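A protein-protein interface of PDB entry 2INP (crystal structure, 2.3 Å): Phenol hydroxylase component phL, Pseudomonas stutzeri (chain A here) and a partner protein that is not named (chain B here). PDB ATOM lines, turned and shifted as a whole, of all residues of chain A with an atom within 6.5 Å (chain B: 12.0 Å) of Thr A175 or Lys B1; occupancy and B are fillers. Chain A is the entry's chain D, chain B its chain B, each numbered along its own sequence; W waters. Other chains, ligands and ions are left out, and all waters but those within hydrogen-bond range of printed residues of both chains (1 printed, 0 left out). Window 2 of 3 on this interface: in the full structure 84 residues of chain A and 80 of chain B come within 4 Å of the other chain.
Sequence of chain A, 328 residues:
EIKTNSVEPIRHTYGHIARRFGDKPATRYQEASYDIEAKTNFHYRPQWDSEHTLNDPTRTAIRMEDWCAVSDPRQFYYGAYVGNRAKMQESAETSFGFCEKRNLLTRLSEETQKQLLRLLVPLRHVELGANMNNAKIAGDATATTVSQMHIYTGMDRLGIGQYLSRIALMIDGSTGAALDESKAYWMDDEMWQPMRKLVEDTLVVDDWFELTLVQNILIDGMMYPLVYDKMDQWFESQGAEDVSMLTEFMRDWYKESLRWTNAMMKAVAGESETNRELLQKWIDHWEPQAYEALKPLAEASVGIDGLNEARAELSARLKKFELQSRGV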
ATOM      1  N   LEU A 169     -18.860 -27.852   3.044  1.00  0.00           N
ATOM      2  CA  LEU A 169     -19.217 -27.798   4.426  1.00  0.00           C
ATOM      3  C   LEU A 169     -20.059 -29.004   4.854  1.00  0.00           C
ATOM      4  O   LEU A 169     -20.038 -29.404   6.015  1.00  0.00           O
ATOM      5  CB  LEU A 169     -19.959 -26.520   4.724  1.00  0.00           C
ATOM      6  CG  LEU A 169     -19.164 -25.230   4.743  1.00  0.00           C
ATOM      7  CD1 LEU A 169     -20.061 -24.082   5.278  1.00  0.00           C
ATOM      8  CD2 LEU A 169     -17.846 -25.400   5.608  1.00  0.00           C
ATOM      9  N   ASP A 172     -17.516 -31.873   5.324  1.00  0.00           N
ATOM     10  CA  ASP A 172     -16.696 -31.784   6.526  1.00  0.00           C
ATOM     11  C   ASP A 172     -17.462 -31.511   7.838  1.00  0.00           C
ATOM     12  O   ASP A 172     -16.857 -31.199   8.913  1.00  0.00           O
ATOM     13  CB  ASP A 172     -15.540 -30.805   6.326  1.00  0.00           C
ATOM     14  CG  ASP A 172     -15.954 -29.315   6.299  1.00  0.00           C
ATOM     15  OD1 ASP A 172     -16.987 -28.913   6.890  1.00  0.00           O
ATOM     16  OD2 ASP A 172     -15.196 -28.516   5.704  1.00  0.00           O
ATOM     17  N   GLY A 173     -18.790 -31.588   7.735  1.00  0.00           N
ATOM     18  CA  GLY A 173     -19.703 -31.296   8.862  1.00  0.00           C
ATOM     19  C   GLY A 173     -19.532 -29.907   9.442  1.00  0.00           C
ATOM     20  O   GLY A 173     -19.597 -29.720  10.670  1.00  0.00           O
ATOM     21  N   SER A 174     -19.283 -28.929   8.570  1.00  0.00           N
ATOM     22  CA  SER A 174     -19.367 -27.493   8.978  1.00  0.00           C
ATOM     23  C   SER A 174     -18.151 -27.028   9.797  1.00  0.00           C
ATOM     24  O   SER A 174     -18.250 -26.152  10.663  1.00  0.00           O
ATOM     25  CB  SER A 174     -20.712 -27.211   9.703  1.00  0.00           C
ATOM     26  OG  SER A 174     -21.160 -25.869   9.539  1.00  0.00           O
ATOM     27  N   THR A 175     -17.003 -27.617   9.482  1.00  0.00           N
ATOM     28  CA  THR A 175     -15.719 -27.266  10.057  1.00  0.00           C
ATOM     29  C   THR A 175     -14.869 -26.366   9.149  1.00  0.00           C
ATOM     30  O   THR A 175     -14.008 -25.569   9.650  1.00  0.00           O
ATOM     31  CB  THR A 175     -14.871 -28.530  10.238  1.00  0.00           C
ATOM     32  OG1 THR A 175     -15.526 -29.432  11.140  1.00  0.00           O
ATOM     33  CG2 THR A 175     -13.549 -28.135  10.879  1.00  0.00           C
ATOM     34  N   GLY A 176     -15.027 -26.529   7.829  1.00  0.00           N
ATOM     35  CA  GLY A 176     -14.214 -25.734   6.923  1.00  0.00           C
ATOM     36  C   GLY A 176     -12.955 -26.415   6.418  1.00  0.00           C
ATOM     37  O   GLY A 176     -12.250 -25.849   5.579  1.00  0.00           O
ATOM     38  N   ALA A 177     -12.713 -27.652   6.866  1.00  0.00           N
ATOM     39  CA  ALA A 177     -11.496 -28.398   6.529  1.00  0.00           C
ATOM     40  C   ALA A 177     -11.495 -28.870   5.082  1.00  0.00           C
ATOM     41  O   ALA A 177     -10.460 -28.843   4.448  1.00  0.00           O
ATOM     42  CB  ALA A 177     -11.313 -29.606   7.497  1.00  0.00           C
ATOM     43  N   ALA A 178     -12.661 -29.297   4.587  1.00  0.00           N
ATOM     44  CA  ALA A 178     -12.906 -29.639   3.160  1.00  0.00           C
ATOM     45  C   ALA A 178     -12.768 -28.421   2.280  1.00  0.00           C
ATOM     46  O   ALA A 178     -12.270 -28.504   1.178  1.00  0.00           O
ATOM     47  CB  ALA A 178     -14.305 -30.248   2.971  1.00  0.00           C
ATOM     48  N   LEU A 179     -13.195 -27.274   2.783  1.00  0.00           N
ATOM     49  CA  LEU A 179     -12.983 -25.998   2.098  1.00  0.00           C
ATOM     50  C   LEU A 179     -11.490 -25.696   1.942  1.00  0.00           C
ATOM     51  O   LEU A 179     -11.042 -25.323   0.814  1.00  0.00           O
ATOM     52  CB  LEU A 179     -13.746 -24.882   2.825  1.00  0.00           C
ATOM     53  CG  LEU A 179     -15.038 -24.280   2.242  1.00  0.00           C
ATOM     54  CD1 LEU A 179     -15.607 -24.982   1.000  1.00  0.00           C
ATOM     55  CD2 LEU A 179     -16.105 -23.996   3.265  1.00  0.00           C
ATOM     56  N   ASP A 180     -10.708 -25.878   3.025  1.00  0.00           N
ATOM     57  CA  ASP A 180      -9.257 -25.715   2.957  1.00  0.00           C
ATOM     58  C   ASP A 180      -8.562 -26.765   2.047  1.00  0.00           C
ATOM     59  O   ASP A 180      -7.637 -26.436   1.296  1.00  0.00           O
ATOM     60  CB  ASP A 180      -8.567 -25.756   4.352  1.00  0.00           C
ATOM     61  CG  ASP A 180      -9.109 -24.740   5.370  1.00  0.00           C
ATOM     62  OD1 ASP A 180      -9.809 -23.755   5.061  1.00  0.00           O
ATOM     63  OD2 ASP A 180      -8.812 -24.947   6.558  1.00  0.00           O
ATOM     64  N   LYS B   1     -13.921 -29.507  14.684  1.00  0.00           N
ATOM     65  CA  LYS B   1     -14.291 -28.262  15.444  1.00  0.00           C
ATOM     66  C   LYS B   1     -15.229 -27.331  14.653  1.00  0.00           C
ATOM     67  O   LYS B   1     -14.730 -26.566  13.797  1.00  0.00           O
ATOM     68  CB  LYS B   1     -12.991 -27.487  15.899  1.00  0.00           C
ATOM     69  N   LYS B   2     -16.540 -27.377  14.973  1.00  0.00           N
ATOM     70  CA  LYS B   2     -17.617 -26.671  14.210  1.00  0.00           C
ATOM     71  C   LYS B   2     -17.471 -25.156  14.084  1.00  0.00           C
ATOM     72  O   LYS B   2     -16.980 -24.498  15.001  1.00  0.00           O
ATOM     73  CB  LYS B   2     -18.996 -26.958  14.783  1.00  0.00           C
ATOM     74  CG  LYS B   2     -19.534 -28.289  14.418  1.00  0.00           C
ATOM     75  CD  LYS B   2     -20.950 -28.121  13.986  1.00  0.00           C
ATOM     76  CE  LYS B   2     -21.554 -29.482  13.617  1.00  0.00           C
ATOM     77  NZ  LYS B   2     -22.782 -29.301  12.766  1.00  0.00           N
ATOM     78  N   LEU B   3     -17.903 -24.595  12.953  1.00  0.00           N
ATOM     79  CA  LEU B   3     -17.677 -23.167  12.681  1.00  0.00           C
ATOM     80  C   LEU B   3     -18.661 -22.246  13.434  1.00  0.00           C
ATOM     81  O   LEU B   3     -19.864 -22.516  13.431  1.00  0.00           O
ATOM     82  CB  LEU B   3     -17.741 -22.885  11.171  1.00  0.00           C
ATOM     83  CG  LEU B   3     -16.552 -23.300  10.320  1.00  0.00           C
ATOM     84  CD1 LEU B   3     -16.905 -23.283   8.820  1.00  0.00           C
ATOM     85  CD2 LEU B   3     -15.295 -22.458  10.652  1.00  0.00           C
ATOM     86  N   ASN B   4     -18.172 -21.161  14.055  1.00  0.00           N
ATOM     87  CA  ASN B   4     -19.140 -20.138  14.558  1.00  0.00           C
ATOM     88  C   ASN B   4     -19.724 -19.256  13.447  1.00  0.00           C
ATOM     89  O   ASN B   4     -19.192 -19.224  12.317  1.00  0.00           O
ATOM     90  CB  ASN B   4     -18.620 -19.288  15.751  1.00  0.00           C
ATOM     91  CG  ASN B   4     -17.421 -18.403  15.394  1.00  0.00           C
ATOM     92  OD1 ASN B   4     -16.526 -18.235  16.211  1.00  0.00           O
ATOM     93  ND2 ASN B   4     -17.394 -17.847  14.173  1.00  0.00           N
ATOM     94  N   LEU B   5     -20.830 -18.589  13.751  1.00  0.00           N
ATOM     95  CA  LEU B   5     -21.488 -17.630  12.799  1.00  0.00           C
ATOM     96  C   LEU B   5     -20.541 -16.716  12.047  1.00  0.00           C
ATOM     97  O   LEU B   5     -20.649 -16.630  10.833  1.00  0.00           O
ATOM     98  CB  LEU B   5     -22.545 -16.766  13.492  1.00  0.00           C
ATOM     99  CG  LEU B   5     -23.720 -17.618  13.936  1.00  0.00           C
ATOM    100  CD1 LEU B   5     -24.800 -16.701  14.447  1.00  0.00           C
ATOM    101  CD2 LEU B   5     -24.216 -18.547  12.767  1.00  0.00           C
ATOM    102  N   LYS B   6     -19.628 -16.046  12.763  1.00  0.00           N
ATOM    103  CA  LYS B   6     -18.573 -15.267  12.123  1.00  0.00           C
ATOM    104  C   LYS B   6     -17.708 -16.023  11.119  1.00  0.00           C
ATOM    105  O   LYS B   6     -17.497 -15.525  10.012  1.00  0.00           O
ATOM    106  CB  LYS B   6     -17.689 -14.550  13.124  1.00  0.00           C
ATOM    107  CG  LYS B   6     -16.534 -13.781  12.438  1.00  0.00           C
ATOM    108  CD  LYS B   6     -15.697 -12.939  13.422  1.00  0.00           C
ATOM    109  CE  LYS B   6     -14.299 -12.530  12.888  1.00  0.00           C
ATOM    110  NZ  LYS B   6     -13.808 -11.435  13.800  1.00  0.00           N
ATOM    111  N   ASP B   7     -17.208 -17.198  11.504  1.00  0.00           N
ATOM    112  CA  ASP B   7     -16.177 -17.917  10.710  1.00  0.00           C
ATOM    113  C   ASP B   7     -16.771 -18.611   9.482  1.00  0.00           C
ATOM    114  O   ASP B   7     -16.081 -18.723   8.453  1.00  0.00           O
ATOM    115  CB  ASP B   7     -15.440 -18.985  11.556  1.00  0.00           C
ATOM    116  CG  ASP B   7     -14.528 -18.384  12.634  1.00  0.00           C
ATOM    117  OD1 ASP B   7     -13.937 -17.293  12.407  1.00  0.00           O
ATOM    118  OD2 ASP B   7     -14.437 -19.027  13.713  1.00  0.00           O
ATOM    119  N   LYS B   8     -18.025 -19.062   9.626  1.00  0.00           N
ATOM    120  CA  LYS B   8     -18.818 -19.699   8.589  1.00  0.00           C
ATOM    121  C   LYS B   8     -19.092 -18.763   7.453  1.00  0.00           C
ATOM    122  O   LYS B   8     -19.051 -19.145   6.293  1.00  0.00           O
ATOM    123  CB  LYS B   8     -20.167 -20.135   9.108  1.00  0.00           C
ATOM    124  CG  LYS B   8     -20.852 -21.023   8.112  1.00  0.00           C
ATOM    125  CD  LYS B   8     -22.074 -21.687   8.697  1.00  0.00           C
ATOM    126  CE  LYS B   8     -23.110 -21.894   7.585  1.00  0.00           C
ATOM    127  NZ  LYS B   8     -23.604 -23.317   7.526  1.00  0.00           N
ATOM    128  N   TYR B   9     -19.375 -17.527   7.809  1.00  0.00           N
ATOM    129  CA  TYR B   9     -19.704 -16.519   6.858  1.00  0.00           C
ATOM    130  C   TYR B   9     -18.474 -16.047   6.112  1.00  0.00           C
ATOM    131  O   TYR B   9     -18.529 -15.768   4.905  1.00  0.00           O
ATOM    132  CB  TYR B   9     -20.359 -15.342   7.581  1.00  0.00           C
ATOM    133  CG  TYR B   9     -20.788 -14.277   6.582  1.00  0.00           C
ATOM    134  CD1 TYR B   9     -20.095 -13.078   6.440  1.00  0.00           C
ATOM    135  CD2 TYR B   9     -21.831 -14.549   5.724  1.00  0.00           C
ATOM    136  CE1 TYR B   9     -20.486 -12.187   5.504  1.00  0.00           C
ATOM    137  CE2 TYR B   9     -22.212 -13.685   4.811  1.00  0.00           C
ATOM    138  CZ  TYR B   9     -21.574 -12.513   4.704  1.00  0.00           C
ATOM    139  OH  TYR B   9     -22.079 -11.710   3.734  1.00  0.00           O
ATOM    140  N   GLN B  10     -17.365 -15.929   6.814  1.00  0.00           N
ATOM    141  CA  GLN B  10     -16.125 -15.623   6.134  1.00  0.00           C
ATOM    142  C   GLN B  10     -15.697 -16.763   5.179  1.00  0.00           C
ATOM    143  O   GLN B  10     -15.144 -16.481   4.095  1.00  0.00           O
ATOM    144  CB  GLN B  10     -15.043 -15.225   7.145  1.00  0.00           C
ATOM    145  CG  GLN B  10     -15.576 -14.041   8.031  1.00  0.00           C
ATOM    146  CD  GLN B  10     -14.518 -13.129   8.707  1.00  0.00           C
ATOM    147  OE1 GLN B  10     -14.882 -12.073   9.268  1.00  0.00           O
ATOM    148  NE2 GLN B  10     -13.243 -13.500   8.642  1.00  0.00           N
ATOM    149  N   TYR B  11     -16.008 -18.018   5.566  1.00  0.00           N
ATOM    150  CA  TYR B  11     -15.856 -19.168   4.716  1.00  0.00           C
ATOM    151  C   TYR B  11     -16.726 -19.066   3.477  1.00  0.00           C
ATOM    152  O   TYR B  11     -16.263 -19.415   2.420  1.00  0.00           O
ATOM    153  CB  TYR B  11     -16.074 -20.496   5.437  1.00  0.00           C
ATOM    154  CG  TYR B  11     -14.747 -21.110   5.897  1.00  0.00           C
ATOM    155  CD1 TYR B  11     -14.446 -21.249   7.273  1.00  0.00           C
ATOM    156  CD2 TYR B  11     -13.791 -21.531   4.967  1.00  0.00           C
ATOM    157  CE1 TYR B  11     -13.230 -21.824   7.702  1.00  0.00           C
ATOM    158  CE2 TYR B  11     -12.579 -22.102   5.363  1.00  0.00           C
ATOM    159  CZ  TYR B  11     -12.300 -22.266   6.744  1.00  0.00           C
ATOM    160  OH  TYR B  11     -11.088 -22.819   7.144  1.00  0.00           O
ATOM    161  N   LEU B  12     -17.924 -18.507   3.607  1.00  0.00           N
ATOM    162  CA  LEU B  12     -18.835 -18.356   2.483  1.00  0.00           C
ATOM    163  C   LEU B  12     -18.596 -17.090   1.653  1.00  0.00           C
ATOM    164  O   LEU B  12     -19.231 -16.896   0.622  1.00  0.00           O
ATOM    165  CB  LEU B  12     -20.280 -18.414   2.941  1.00  0.00           C
ATOM    166  CG  LEU B  12     -20.680 -19.769   3.541  1.00  0.00           C
ATOM    167  CD1 LEU B  12     -22.054 -19.708   4.221  1.00  0.00           C
ATOM    168  CD2 LEU B  12     -20.614 -20.902   2.480  1.00  0.00           C
ATOM    169  N   ASP B  15     -13.212 -16.672   2.018  1.00  0.00           N
ATOM    170  CA  ASP B  15     -12.426 -17.860   1.664  1.00  0.00           C
ATOM    171  C   ASP B  15     -12.470 -18.205   0.147  1.00  0.00           C
ATOM    172  O   ASP B  15     -11.586 -18.913  -0.353  1.00  0.00           O
ATOM    173  CB  ASP B  15     -12.770 -19.070   2.565  1.00  0.00           C
ATOM    174  CG  ASP B  15     -11.856 -20.289   2.300  1.00  0.00           C
ATOM    175  OD1 ASP B  15     -12.348 -21.411   1.985  1.00  0.00           O
ATOM    176  OD2 ASP B  15     -10.612 -20.120   2.388  1.00  0.00           O
HETATM  177  O   HOH W   1      -9.252 -22.094   3.146  1.00  0.00           O
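Of chain B, only Lys B1 (3.5 Å) and Leu B3 (3.5 Å) come within 4 Å of Thr A175.
Of chain A, only Thr A175 comes within 4 Å of Lys B1.
Of chain B, only Leu B3 (3.96 Å) comes within 4 Å of Leu A169.
Gly A173 touches just one residue of chain B: Lys B2 (3.5 Å).
Of chain B, only Lys B2 (3.6 Å) and Leu B3 (2.8 Å) come within 4 Å of Ser A174.
Gly A176 touches just these residues of chain B: Leu B3 (3.9 Å) and Tyr B11 (3.6 Å).
No residue of chain B comes within 4 Å of Ala A177.
Of the printed residues of chain A, Tyr B11 touches Gly A176, Leu A179 and Asp A180.
Printed residues of chain A within 4 Å of Asp B15: Leu A179.
Printed residues of chain B within 4 Å of Leu A179: Tyr B11 (3.8 Å) and Asp B15 (3.8 Å).
Leu B12 touches none of the printed residues of chain A.
The nearest printed residue of chain B that does not touch Asp A180 is Asp B15 (4.6 Å).
Water W1 lies within hydrogen-bond range of the side-chain carboxylate (OD2) of Asp B15 (2.5 Å) and the side-chain carboxylate (OD1) of Asp A180 (2.6 Å).
The backbone NH of Ser A174 sits at hydrogen-bond distance from the backbone carbonyl oxygen of Leu A169.
The side-chain carboxylate (OD1) of Asp A172 is in hydrogen-bond range of the backbone NH (N) of Thr A175 (2.9 Å).
The side-chain carboxylate (OD2) of Asp A172 sits at hydrogen-bond distance from the backbone NH (N) of Gly A176, 2.9 Å away.
The side-chain carboxylate (OD1) of Asp A172 sits at hydrogen-bond distance from the backbone NH (N) of Ser A174 (2.8 Å).
The backbone carbonyl oxygen (O) of Gln B10 lies within hydrogen-bond range of the backbone NH (N) of Asp B15, 2.8 Å away.
OH of Tyr B11 lies within hydrogen-bond range of OD1 of Asp A180 (2.6 Å).
The backbone NH (N) of Leu B3 lies within hydrogen-bond range of the backbone carbonyl oxygen (O) of Ser A174 (2.8 Å).
CD2 of Leu A169 touches CD1 of Leu B3, 3.96 Å away.
O of Gly A173 touches CE of Lys B2, at 3.5 Å.
O of Ser A174 touches CA of Lys B2 (3.6 Å).
O of Lys B1 touches CG2 of Thr A175 (3.5 Å).
Thr A175 touches Leu B3 (O to CG, 3.5 Å).
Gly A176 touches Leu B3 (N to CD1, 3.9 Å).
Gly A176 touches Tyr B11.
Leu A179 touches Tyr B11.
Leu A179 touches Asp B15 (CB to OD1, 3.8 Å).
Hydrophobic or aromatic side chains of chain B that line the printed part of chain A: Leu B3 and Tyr B11.
Of the 10 printed residues of chain A, 7 touch a printed residue of chain B.
Hydrophobic or aromatic side chains of chain A within 4 Å of the printed part of chain B: Leu A169 and Leu A179.
Among the printed residues, 11 pairs touch across the chains.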
